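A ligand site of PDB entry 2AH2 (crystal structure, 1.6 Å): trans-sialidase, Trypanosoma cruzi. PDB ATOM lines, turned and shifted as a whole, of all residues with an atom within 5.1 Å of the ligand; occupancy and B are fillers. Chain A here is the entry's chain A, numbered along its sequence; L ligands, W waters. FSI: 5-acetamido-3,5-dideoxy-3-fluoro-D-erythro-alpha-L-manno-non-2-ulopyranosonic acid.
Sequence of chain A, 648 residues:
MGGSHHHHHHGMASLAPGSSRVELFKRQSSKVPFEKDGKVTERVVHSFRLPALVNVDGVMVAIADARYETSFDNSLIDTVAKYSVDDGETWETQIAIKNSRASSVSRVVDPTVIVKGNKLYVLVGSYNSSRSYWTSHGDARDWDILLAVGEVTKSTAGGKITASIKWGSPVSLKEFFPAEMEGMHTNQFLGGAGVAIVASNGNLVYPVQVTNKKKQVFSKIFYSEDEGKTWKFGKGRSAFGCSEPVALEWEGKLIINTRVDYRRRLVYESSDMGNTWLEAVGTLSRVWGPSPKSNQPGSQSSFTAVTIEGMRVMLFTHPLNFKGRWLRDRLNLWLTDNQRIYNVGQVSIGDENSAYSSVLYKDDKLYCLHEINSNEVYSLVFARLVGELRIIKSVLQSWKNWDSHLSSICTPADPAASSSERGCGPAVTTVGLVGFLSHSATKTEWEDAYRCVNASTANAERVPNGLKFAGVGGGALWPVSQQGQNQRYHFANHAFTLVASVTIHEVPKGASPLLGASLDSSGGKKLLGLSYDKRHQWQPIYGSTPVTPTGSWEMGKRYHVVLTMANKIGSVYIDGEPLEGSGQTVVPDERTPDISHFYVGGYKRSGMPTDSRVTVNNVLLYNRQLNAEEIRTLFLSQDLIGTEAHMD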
ATOM      1  N   ARG A  49      23.423   7.064 -26.143  1.00  0.00           N
ATOM      2  CA  ARG A  49      22.180   7.705 -25.759  1.00  0.00           C
ATOM      3  C   ARG A  49      21.280   7.847 -26.992  1.00  0.00           C
ATOM      4  O   ARG A  49      21.659   7.527 -28.089  1.00  0.00           O
ATOM      5  CB  ARG A  49      22.409   9.063 -25.099  1.00  0.00           C
ATOM      6  CG  ARG A  49      23.097   8.991 -23.683  1.00  0.00           C
ATOM      7  CD  ARG A  49      22.715  10.182 -22.840  1.00  0.00           C
ATOM      8  NE  ARG A  49      21.272  10.156 -22.608  1.00  0.00           N
ATOM      9  CZ  ARG A  49      20.516  11.137 -22.164  1.00  0.00           C
ATOM     10  NH1 ARG A  49      19.200  10.921 -22.025  1.00  0.00           N
ATOM     11  NH2 ARG A  49      21.035  12.300 -21.823  1.00  0.00           N
ATOM     12  N   LEU A  50      20.072   8.336 -26.768  1.00  0.00           N
ATOM     13  CA  LEU A  50      19.230   8.763 -27.879  1.00  0.00           C
ATOM     14  C   LEU A  50      18.787   7.593 -28.796  1.00  0.00           C
ATOM     15  O   LEU A  50      18.875   7.671 -30.021  1.00  0.00           O
ATOM     16  CB  LEU A  50      19.873   9.895 -28.683  1.00  0.00           C
ATOM     17  CG  LEU A  50      19.614  11.355 -28.235  1.00  0.00           C
ATOM     18  CD1 LEU A  50      18.227  11.782 -28.481  1.00  0.00           C
ATOM     19  CD2 LEU A  50      19.988  11.491 -26.733  1.00  0.00           C
ATOM     20  N   ASP A  65      23.122   8.187 -30.375  1.00  0.00           N
ATOM     21  CA  ASP A  65      24.349   8.944 -30.150  1.00  0.00           C
ATOM     22  C   ASP A  65      25.462   8.038 -29.687  1.00  0.00           C
ATOM     23  O   ASP A  65      25.243   7.267 -28.778  1.00  0.00           O
ATOM     24  CB  ASP A  65      24.194   9.856 -28.971  1.00  0.00           C
ATOM     25  CG  ASP A  65      23.409  11.146 -29.196  1.00  0.00           C
ATOM     26  OD1 ASP A  65      22.877  11.484 -30.271  1.00  0.00           O
ATOM     27  OD2 ASP A  65      23.384  11.947 -28.178  1.00  0.00           O
ATOM     28  N   ARG A  67      28.564   8.920 -27.836  1.00  0.00           N
ATOM     29  CA  ARG A  67      29.229   9.970 -27.053  1.00  0.00           C
ATOM     30  C   ARG A  67      30.600   9.426 -26.630  1.00  0.00           C
ATOM     31  O   ARG A  67      30.752   8.682 -25.668  1.00  0.00           O
ATOM     32  CB  ARG A  67      28.368  10.426 -25.876  1.00  0.00           C
ATOM     33  CG  ARG A  67      26.937  10.798 -26.267  1.00  0.00           C
ATOM     34  CD  ARG A  67      26.211  11.643 -25.250  1.00  0.00           C
ATOM     35  NE  ARG A  67      24.875  12.015 -25.724  1.00  0.00           N
ATOM     36  CZ  ARG A  67      24.079  12.847 -25.095  1.00  0.00           C
ATOM     37  NH1 ARG A  67      24.424  13.295 -23.871  1.00  0.00           N
ATOM     38  NH2 ARG A  67      22.918  13.177 -25.624  1.00  0.00           N
ATOM     39  N   ASP A  73      26.285  16.402 -22.568  1.00  0.00           N
ATOM     40  CA  ASP A  73      25.480  16.585 -23.811  1.00  0.00           C
ATOM     41  C   ASP A  73      26.341  17.291 -24.835  1.00  0.00           C
ATOM     42  O   ASP A  73      26.292  17.016 -26.010  1.00  0.00           O
ATOM     43  CB  ASP A  73      24.241  17.462 -23.573  1.00  0.00           C
ATOM     44  CG  ASP A  73      23.110  16.765 -22.744  1.00  0.00           C
ATOM     45  OD1 ASP A  73      22.985  15.479 -22.680  1.00  0.00           O
ATOM     46  OD2 ASP A  73      22.253  17.483 -22.143  1.00  0.00           O
ATOM     47  N   ASN A  74      27.112  18.251 -24.366  1.00  0.00           N
ATOM     48  CA  ASN A  74      27.861  19.154 -25.235  1.00  0.00           C
ATOM     49  C   ASN A  74      29.318  18.704 -25.334  1.00  0.00           C
ATOM     50  O   ASN A  74      30.238  19.340 -24.788  1.00  0.00           O
ATOM     51  CB  ASN A  74      27.692  20.561 -24.679  1.00  0.00           C
ATOM     52  CG  ASN A  74      26.204  20.913 -24.333  1.00  0.00           C
ATOM     53  OD1 ASN A  74      25.913  21.429 -23.224  1.00  0.00           O
ATOM     54  ND2 ASN A  74      25.302  20.689 -25.262  1.00  0.00           N
ATOM     55  N   VAL A 109      23.570  15.699 -33.097  1.00  0.00           N
ATOM     56  CA  VAL A 109      22.766  15.477 -31.908  1.00  0.00           C
ATOM     57  C   VAL A 109      21.323  15.141 -32.164  1.00  0.00           C
ATOM     58  O   VAL A 109      20.701  15.588 -33.125  1.00  0.00           O
ATOM     59  CB  VAL A 109      22.817  16.702 -30.925  1.00  0.00           C
ATOM     60  CG1 VAL A 109      24.209  17.052 -30.513  1.00  0.00           C
ATOM     61  CG2 VAL A 109      22.136  17.909 -31.524  1.00  0.00           C
ATOM     62  N   ASP A 110      20.802  14.324 -31.263  1.00  0.00           N
ATOM     63  CA  ASP A 110      19.372  14.007 -31.146  1.00  0.00           C
ATOM     64  C   ASP A 110      18.802  13.473 -32.453  1.00  0.00           C
ATOM     65  O   ASP A 110      17.815  13.997 -32.972  1.00  0.00           O
ATOM     66  CB  ASP A 110      18.548  15.172 -30.614  1.00  0.00           C
ATOM     67  CG  ASP A 110      18.814  15.458 -29.158  1.00  0.00           C
ATOM     68  OD1 ASP A 110      18.011  16.211 -28.572  1.00  0.00           O
ATOM     69  OD2 ASP A 110      19.805  14.933 -28.518  1.00  0.00           O
ATOM     70  N   TYR A 133      24.246  24.427 -23.112  1.00  0.00           N
ATOM     71  CA  TYR A 133      22.951  23.832 -23.451  1.00  0.00           C
ATOM     72  C   TYR A 133      22.257  24.613 -24.561  1.00  0.00           C
ATOM     73  O   TYR A 133      22.264  25.848 -24.586  1.00  0.00           O
ATOM     74  CB  TYR A 133      22.114  23.755 -22.181  1.00  0.00           C
ATOM     75  CG  TYR A 133      20.754  23.151 -22.415  1.00  0.00           C
ATOM     76  CD1 TYR A 133      20.627  21.796 -22.705  1.00  0.00           C
ATOM     77  CD2 TYR A 133      19.607  23.914 -22.392  1.00  0.00           C
ATOM     78  CE1 TYR A 133      19.406  21.225 -22.945  1.00  0.00           C
ATOM     79  CE2 TYR A 133      18.384  23.357 -22.633  1.00  0.00           C
ATOM     80  CZ  TYR A 133      18.276  22.025 -22.920  1.00  0.00           C
ATOM     81  OH  TYR A 133      17.046  21.460 -23.151  1.00  0.00           O
ATOM     82  N   TRP A 134      21.642  23.906 -25.514  1.00  0.00           N
ATOM     83  CA  TRP A 134      21.142  24.571 -26.700  1.00  0.00           C
ATOM     84  C   TRP A 134      20.167  25.725 -26.453  1.00  0.00           C
ATOM     85  O   TRP A 134      20.289  26.738 -27.105  1.00  0.00           O
ATOM     86  CB  TRP A 134      20.637  23.558 -27.720  1.00  0.00           C
ATOM     87  CG  TRP A 134      19.247  23.031 -27.432  1.00  0.00           C
ATOM     88  CD1 TRP A 134      18.862  22.188 -26.419  1.00  0.00           C
ATOM     89  CD2 TRP A 134      18.074  23.326 -28.184  1.00  0.00           C
ATOM     90  NE1 TRP A 134      17.508  21.934 -26.515  1.00  0.00           N
ATOM     91  CE2 TRP A 134      17.002  22.618 -27.591  1.00  0.00           C
ATOM     92  CE3 TRP A 134      17.813  24.108 -29.326  1.00  0.00           C
ATOM     93  CZ2 TRP A 134      15.709  22.681 -28.097  1.00  0.00           C
ATOM     94  CZ3 TRP A 134      16.535  24.159 -29.831  1.00  0.00           C
ATOM     95  CH2 TRP A 134      15.506  23.441 -29.224  1.00  0.00           C
ATOM     96  N   THR A 135      19.273  25.629 -25.470  1.00  0.00           N
ATOM     97  CA  THR A 135      18.330  26.702 -25.292  1.00  0.00           C
ATOM     98  C   THR A 135      18.940  27.903 -24.591  1.00  0.00           C
ATOM     99  O   THR A 135      18.297  28.916 -24.488  1.00  0.00           O
ATOM    100  CB  THR A 135      17.027  26.262 -24.604  1.00  0.00           C
ATOM    101  OG1 THR A 135      17.274  26.026 -23.211  1.00  0.00           O
ATOM    102  CG2 THR A 135      16.464  24.967 -25.212  1.00  0.00           C
ATOM    103  N   LEU A 190      15.554  21.622 -33.494  1.00  0.00           N
ATOM    104  CA  LEU A 190      16.043  20.259 -33.457  1.00  0.00           C
ATOM    105  C   LEU A 190      14.873  19.287 -33.611  1.00  0.00           C
ATOM    106  O   LEU A 190      13.733  19.628 -33.294  1.00  0.00           O
ATOM    107  CB  LEU A 190      16.697  19.956 -32.120  1.00  0.00           C
ATOM    108  CG  LEU A 190      17.940  20.807 -31.811  1.00  0.00           C
ATOM    109  CD1 LEU A 190      18.369  20.566 -30.372  1.00  0.00           C
ATOM    110  CD2 LEU A 190      19.098  20.496 -32.748  1.00  0.00           C
ATOM    111  N   GLN A 209      11.335  20.823 -32.029  1.00  0.00           N
ATOM    112  CA  GLN A 209      11.414  21.765 -30.948  1.00  0.00           C
ATOM    113  C   GLN A 209      12.247  22.941 -31.473  1.00  0.00           C
ATOM    114  O   GLN A 209      13.321  22.766 -32.074  1.00  0.00           O
ATOM    115  CB  GLN A 209      12.035  21.130 -29.711  1.00  0.00           C
ATOM    116  CG  GLN A 209      13.339  20.404 -29.950  1.00  0.00           C
ATOM    117  CD  GLN A 209      13.814  19.629 -28.718  1.00  0.00           C
ATOM    118  OE1 GLN A 209      13.468  19.995 -27.577  1.00  0.00           O
ATOM    119  NE2 GLN A 209      14.684  18.653 -28.941  1.00  0.00           N
ATOM    120  N   SER A 243       8.592  21.043 -25.320  1.00  0.00           N
ATOM    121  CA  SER A 243       9.809  20.666 -26.022  1.00  0.00           C
ATOM    122  C   SER A 243       9.704  19.223 -26.502  1.00  0.00           C
ATOM    123  O   SER A 243       8.706  18.527 -26.274  1.00  0.00           O
ATOM    124  CB  SER A 243      11.041  20.855 -25.125  1.00  0.00           C
ATOM    125  OG  SER A 243      10.972  19.918 -24.066  1.00  0.00           O
ATOM    126  N   GLU A 244      10.785  18.821 -27.177  1.00  0.00           N
ATOM    127  CA  GLU A 244      11.059  17.434 -27.582  1.00  0.00           C
ATOM    128  C   GLU A 244       9.769  16.662 -27.954  1.00  0.00           C
ATOM    129  O   GLU A 244       9.420  15.648 -27.322  1.00  0.00           O
ATOM    130  CB  GLU A 244      11.789  16.700 -26.457  1.00  0.00           C
ATOM    131  CG  GLU A 244      12.728  15.665 -27.027  1.00  0.00           C
ATOM    132  CD  GLU A 244      13.713  15.065 -26.077  1.00  0.00           C
ATOM    133  OE1 GLU A 244      13.358  14.881 -24.907  1.00  0.00           O
ATOM    134  OE2 GLU A 244      14.837  14.703 -26.566  1.00  0.00           O
ATOM    135  N   ARG A 259       6.982  17.067 -24.378  1.00  0.00           N
ATOM    136  CA  ARG A 259       7.646  17.114 -23.093  1.00  0.00           C
ATOM    137  C   ARG A 259       7.447  18.517 -22.530  1.00  0.00           C
ATOM    138  O   ARG A 259       7.659  19.513 -23.205  1.00  0.00           O
ATOM    139  CB  ARG A 259       9.123  16.874 -23.327  1.00  0.00           C
ATOM    140  CG  ARG A 259      10.077  17.125 -22.143  1.00  0.00           C
ATOM    141  CD  ARG A 259      11.467  16.731 -22.448  1.00  0.00           C
ATOM    142  NE  ARG A 259      12.386  17.071 -21.406  1.00  0.00           N
ATOM    143  CZ  ARG A 259      13.612  16.646 -21.365  1.00  0.00           C
ATOM    144  NH1 ARG A 259      14.074  15.830 -22.274  1.00  0.00           N
ATOM    145  NH2 ARG A 259      14.396  17.048 -20.413  1.00  0.00           N
ATOM    146  N   GLY A 298      11.127  16.411 -17.595  1.00  0.00           N
ATOM    147  CA  GLY A 298      10.478  15.442 -18.435  1.00  0.00           C
ATOM    148  C   GLY A 298      11.467  14.551 -19.208  1.00  0.00           C
ATOM    149  O   GLY A 298      12.631  14.451 -18.875  1.00  0.00           O
ATOM    150  N   TRP A 326      17.075  14.331 -13.460  1.00  0.00           N
ATOM    151  CA  TRP A 326      17.093  13.659 -14.737  1.00  0.00           C
ATOM    152  C   TRP A 326      17.351  12.172 -14.583  1.00  0.00           C
ATOM    153  O   TRP A 326      17.540  11.485 -15.584  1.00  0.00           O
ATOM    154  CB  TRP A 326      18.088  14.296 -15.710  1.00  0.00           C
ATOM    155  CG  TRP A 326      17.720  15.649 -16.108  1.00  0.00           C
ATOM    156  CD1 TRP A 326      17.061  16.015 -17.254  1.00  0.00           C
ATOM    157  CD2 TRP A 326      18.007  16.858 -15.415  1.00  0.00           C
ATOM    158  NE1 TRP A 326      16.881  17.368 -17.283  1.00  0.00           N
ATOM    159  CE2 TRP A 326      17.467  17.920 -16.185  1.00  0.00           C
ATOM    160  CE3 TRP A 326      18.701  17.160 -14.273  1.00  0.00           C
ATOM    161  CZ2 TRP A 326      17.544  19.254 -15.790  1.00  0.00           C
ATOM    162  CZ3 TRP A 326      18.740  18.481 -13.841  1.00  0.00           C
ATOM    163  CH2 TRP A 326      18.192  19.500 -14.613  1.00  0.00           C
ATOM    164  N   ARG A 328      15.394   9.585 -13.775  1.00  0.00           N
ATOM    165  CA  ARG A 328      14.374   9.017 -14.651  1.00  0.00           C
ATOM    166  C   ARG A 328      14.425   7.505 -14.707  1.00  0.00           C
ATOM    167  O   ARG A 328      14.457   6.855 -15.771  1.00  0.00           O
ATOM    168  CB  ARG A 328      14.488   9.706 -16.013  1.00  0.00           C
ATOM    169  CG  ARG A 328      13.987  11.145 -15.948  1.00  0.00           C
ATOM    170  CD  ARG A 328      14.159  11.934 -17.223  1.00  0.00           C
ATOM    171  NE  ARG A 328      15.583  12.059 -17.545  1.00  0.00           N
ATOM    172  CZ  ARG A 328      16.077  12.681 -18.583  1.00  0.00           C
ATOM    173  NH1 ARG A 328      15.274  13.381 -19.404  1.00  0.00           N
ATOM    174  NH2 ARG A 328      17.385  12.647 -18.818  1.00  0.00           N
ATOM    175  N   TYR A 356      15.519   7.622 -21.947  1.00  0.00           N
ATOM    176  CA  TYR A 356      15.059   7.666 -23.323  1.00  0.00           C
ATOM    177  C   TYR A 356      14.851   6.232 -23.862  1.00  0.00           C
ATOM    178  O   TYR A 356      15.507   5.287 -23.431  1.00  0.00           O
ATOM    179  CB  TYR A 356      16.051   8.395 -24.164  1.00  0.00           C
ATOM    180  CG  TYR A 356      16.143   9.918 -24.045  1.00  0.00           C
ATOM    181  CD1 TYR A 356      15.732  10.625 -22.902  1.00  0.00           C
ATOM    182  CD2 TYR A 356      16.626  10.653 -25.122  1.00  0.00           C
ATOM    183  CE1 TYR A 356      15.882  12.006 -22.831  1.00  0.00           C
ATOM    184  CE2 TYR A 356      16.778  11.985 -25.071  1.00  0.00           C
ATOM    185  CZ  TYR A 356      16.415  12.691 -23.915  1.00  0.00           C
ATOM    186  OH  TYR A 356      16.514  14.080 -23.918  1.00  0.00           O
HETATM  187  C1  FSI L   1      17.513  14.478 -21.793  1.00  0.00           C
HETATM  188  F1  FSI L   1      19.883  15.048 -23.066  1.00  0.00           F
HETATM  189  C2  FSI L   1      17.575  14.777 -23.278  1.00  0.00           C
HETATM  190  C3  FSI L   1      18.936  14.517 -23.854  1.00  0.00           C
HETATM  191  C4  FSI L   1      19.079  15.196 -25.204  1.00  0.00           C
HETATM  192  O4  FSI L   1      20.356  14.982 -25.706  1.00  0.00           O
HETATM  193  C5  FSI L   1      18.911  16.742 -25.087  1.00  0.00           C
HETATM  194  N5  FSI L   1      19.171  17.392 -26.266  1.00  0.00           N
HETATM  195  C6  FSI L   1      17.442  16.817 -24.635  1.00  0.00           C
HETATM  196  O6  FSI L   1      17.261  16.149 -23.359  1.00  0.00           O
HETATM  197  C7  FSI L   1      16.868  18.217 -24.497  1.00  0.00           C
HETATM  198  O7  FSI L   1      17.280  18.818 -23.294  1.00  0.00           O
HETATM  199  C8  FSI L   1      15.321  18.202 -24.636  1.00  0.00           C
HETATM  200  O8  FSI L   1      14.987  17.855 -25.958  1.00  0.00           O
HETATM  201  C9  FSI L   1      14.678  19.534 -24.275  1.00  0.00           C
HETATM  202  O9  FSI L   1      15.140  20.501 -25.208  1.00  0.00           O
HETATM  203  C10 FSI L   1      20.015  18.438 -26.411  1.00  0.00           C
HETATM  204  O10 FSI L   1      20.545  19.020 -25.448  1.00  0.00           O
HETATM  205  C11 FSI L   1      20.310  18.966 -27.800  1.00  0.00           C
HETATM  206  O1A FSI L   1      16.647  15.080 -21.085  1.00  0.00           O
HETATM  207  O1B FSI L   1      18.286  13.641 -21.299  1.00  0.00           O
HETATM  208  O   HOH W   1      14.163  22.683 -23.435  1.00  0.00           O
HETATM  209  O   HOH W   2      22.313  21.036 -25.722  1.00  0.00           O
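OH of Tyr 356 sits at hydrogen-bond distance from NH1 of Arg 259 (3.4 Å). NE1 of Trp 134 sits at hydrogen-bond distance from OH of Tyr 133 (3.4 Å). N of Ser 243 sits at hydrogen-bond distance from O of Arg 259 (2.8 Å). N of Glu 244 lies within hydrogen-bond range of OE1 of Gln 209, 3.0 Å away. The backbone NH of Leu 190 lies within hydrogen-bond range of the backbone carbonyl oxygen of Gln 209 (2.9 Å). The guanidinium group (NH2) of Arg 49 is in salt-bridge range of the side-chain carboxylate (OD1) of Asp 73, 3.8 Å away. The backbone carbonyl oxygen (O) of Arg 49 is in hydrogen-bond range of the backbone NH (N) of Asp 65, at 2.8 Å. NH1 of Arg 67 is in salt-bridge range of OD1 of Asp 73 (2.9 Å).
The side-chain hydroxyl of Tyr 356 is covalently linked to a carbon (C2) of the ligand (1.4 Å). An oxygen (O7) of the ligand lies within hydrogen-bond range of the side-chain hydroxyl (OH) of Tyr 133 (2.7 Å). The guanidinium group (NH1) of Arg 328 is in salt-bridge range of an oxygen (O1A) of the ligand, 2.8 Å away. OD1 of Asp 110 sits at hydrogen-bond distance from N5 of the ligand, 2.8 Å away. An oxygen (O1A) of the ligand lies within salt-bridge range of the guanidinium group (NH1) of Arg 259, 2.9 Å away. The side-chain amide oxygen (OE1) of Gln 209 is in hydrogen-bond range of an oxygen (O9) of the ligand. O1B of the ligand is in salt-bridge range of NH1 of Arg 49 (3.0 Å). O9 of the ligand lies within hydrogen-bond range of NE1 of Trp 134 (3.1 Å). An oxygen (O8) of the ligand lies close to the side-chain carboxylate (OE2) of Glu 244. NH2 of Arg 67 lies within hydrogen-bond range of O4 of the ligand, 3.1 Å away.
The side-chain carboxylate (OD1) of Asp 73 lies close to a fluorine (F1) of the ligand, 3.2 Å away. Residues that only touch the ligand: Leu 190 (3.6 Å), Leu 50 (3.7 Å), Ser 243 (3.7 Å) and Trp 326 (3.97 Å). Hydrophobic or aromatic side chains within 4 Å of the ligand: Leu 50, Tyr 133, Trp 134, Leu 190, Trp 326 and Tyr 356. 15 residues have an atom within 4 Å of the ligand: Arg 49, Leu 50, Arg 67, Asp 73, Asp 110, Tyr 133, Trp 134, Leu 190, Gln 209, Ser 243, Glu 244, Arg 259, Trp 326, Arg 328 and Tyr 356. The nearest printed residue that does not touch the ligand is Val 109 (4.3 Å).
Water W2 lies within hydrogen-bond range of an oxygen (O10) of the ligand, the backbone NH of Trp 134 and the side-chain amide nitrogen of Asn 74. Water W1 bridges O9 of the ligand (3.0 Å) and OH of Tyr 133 (3.1 Å).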
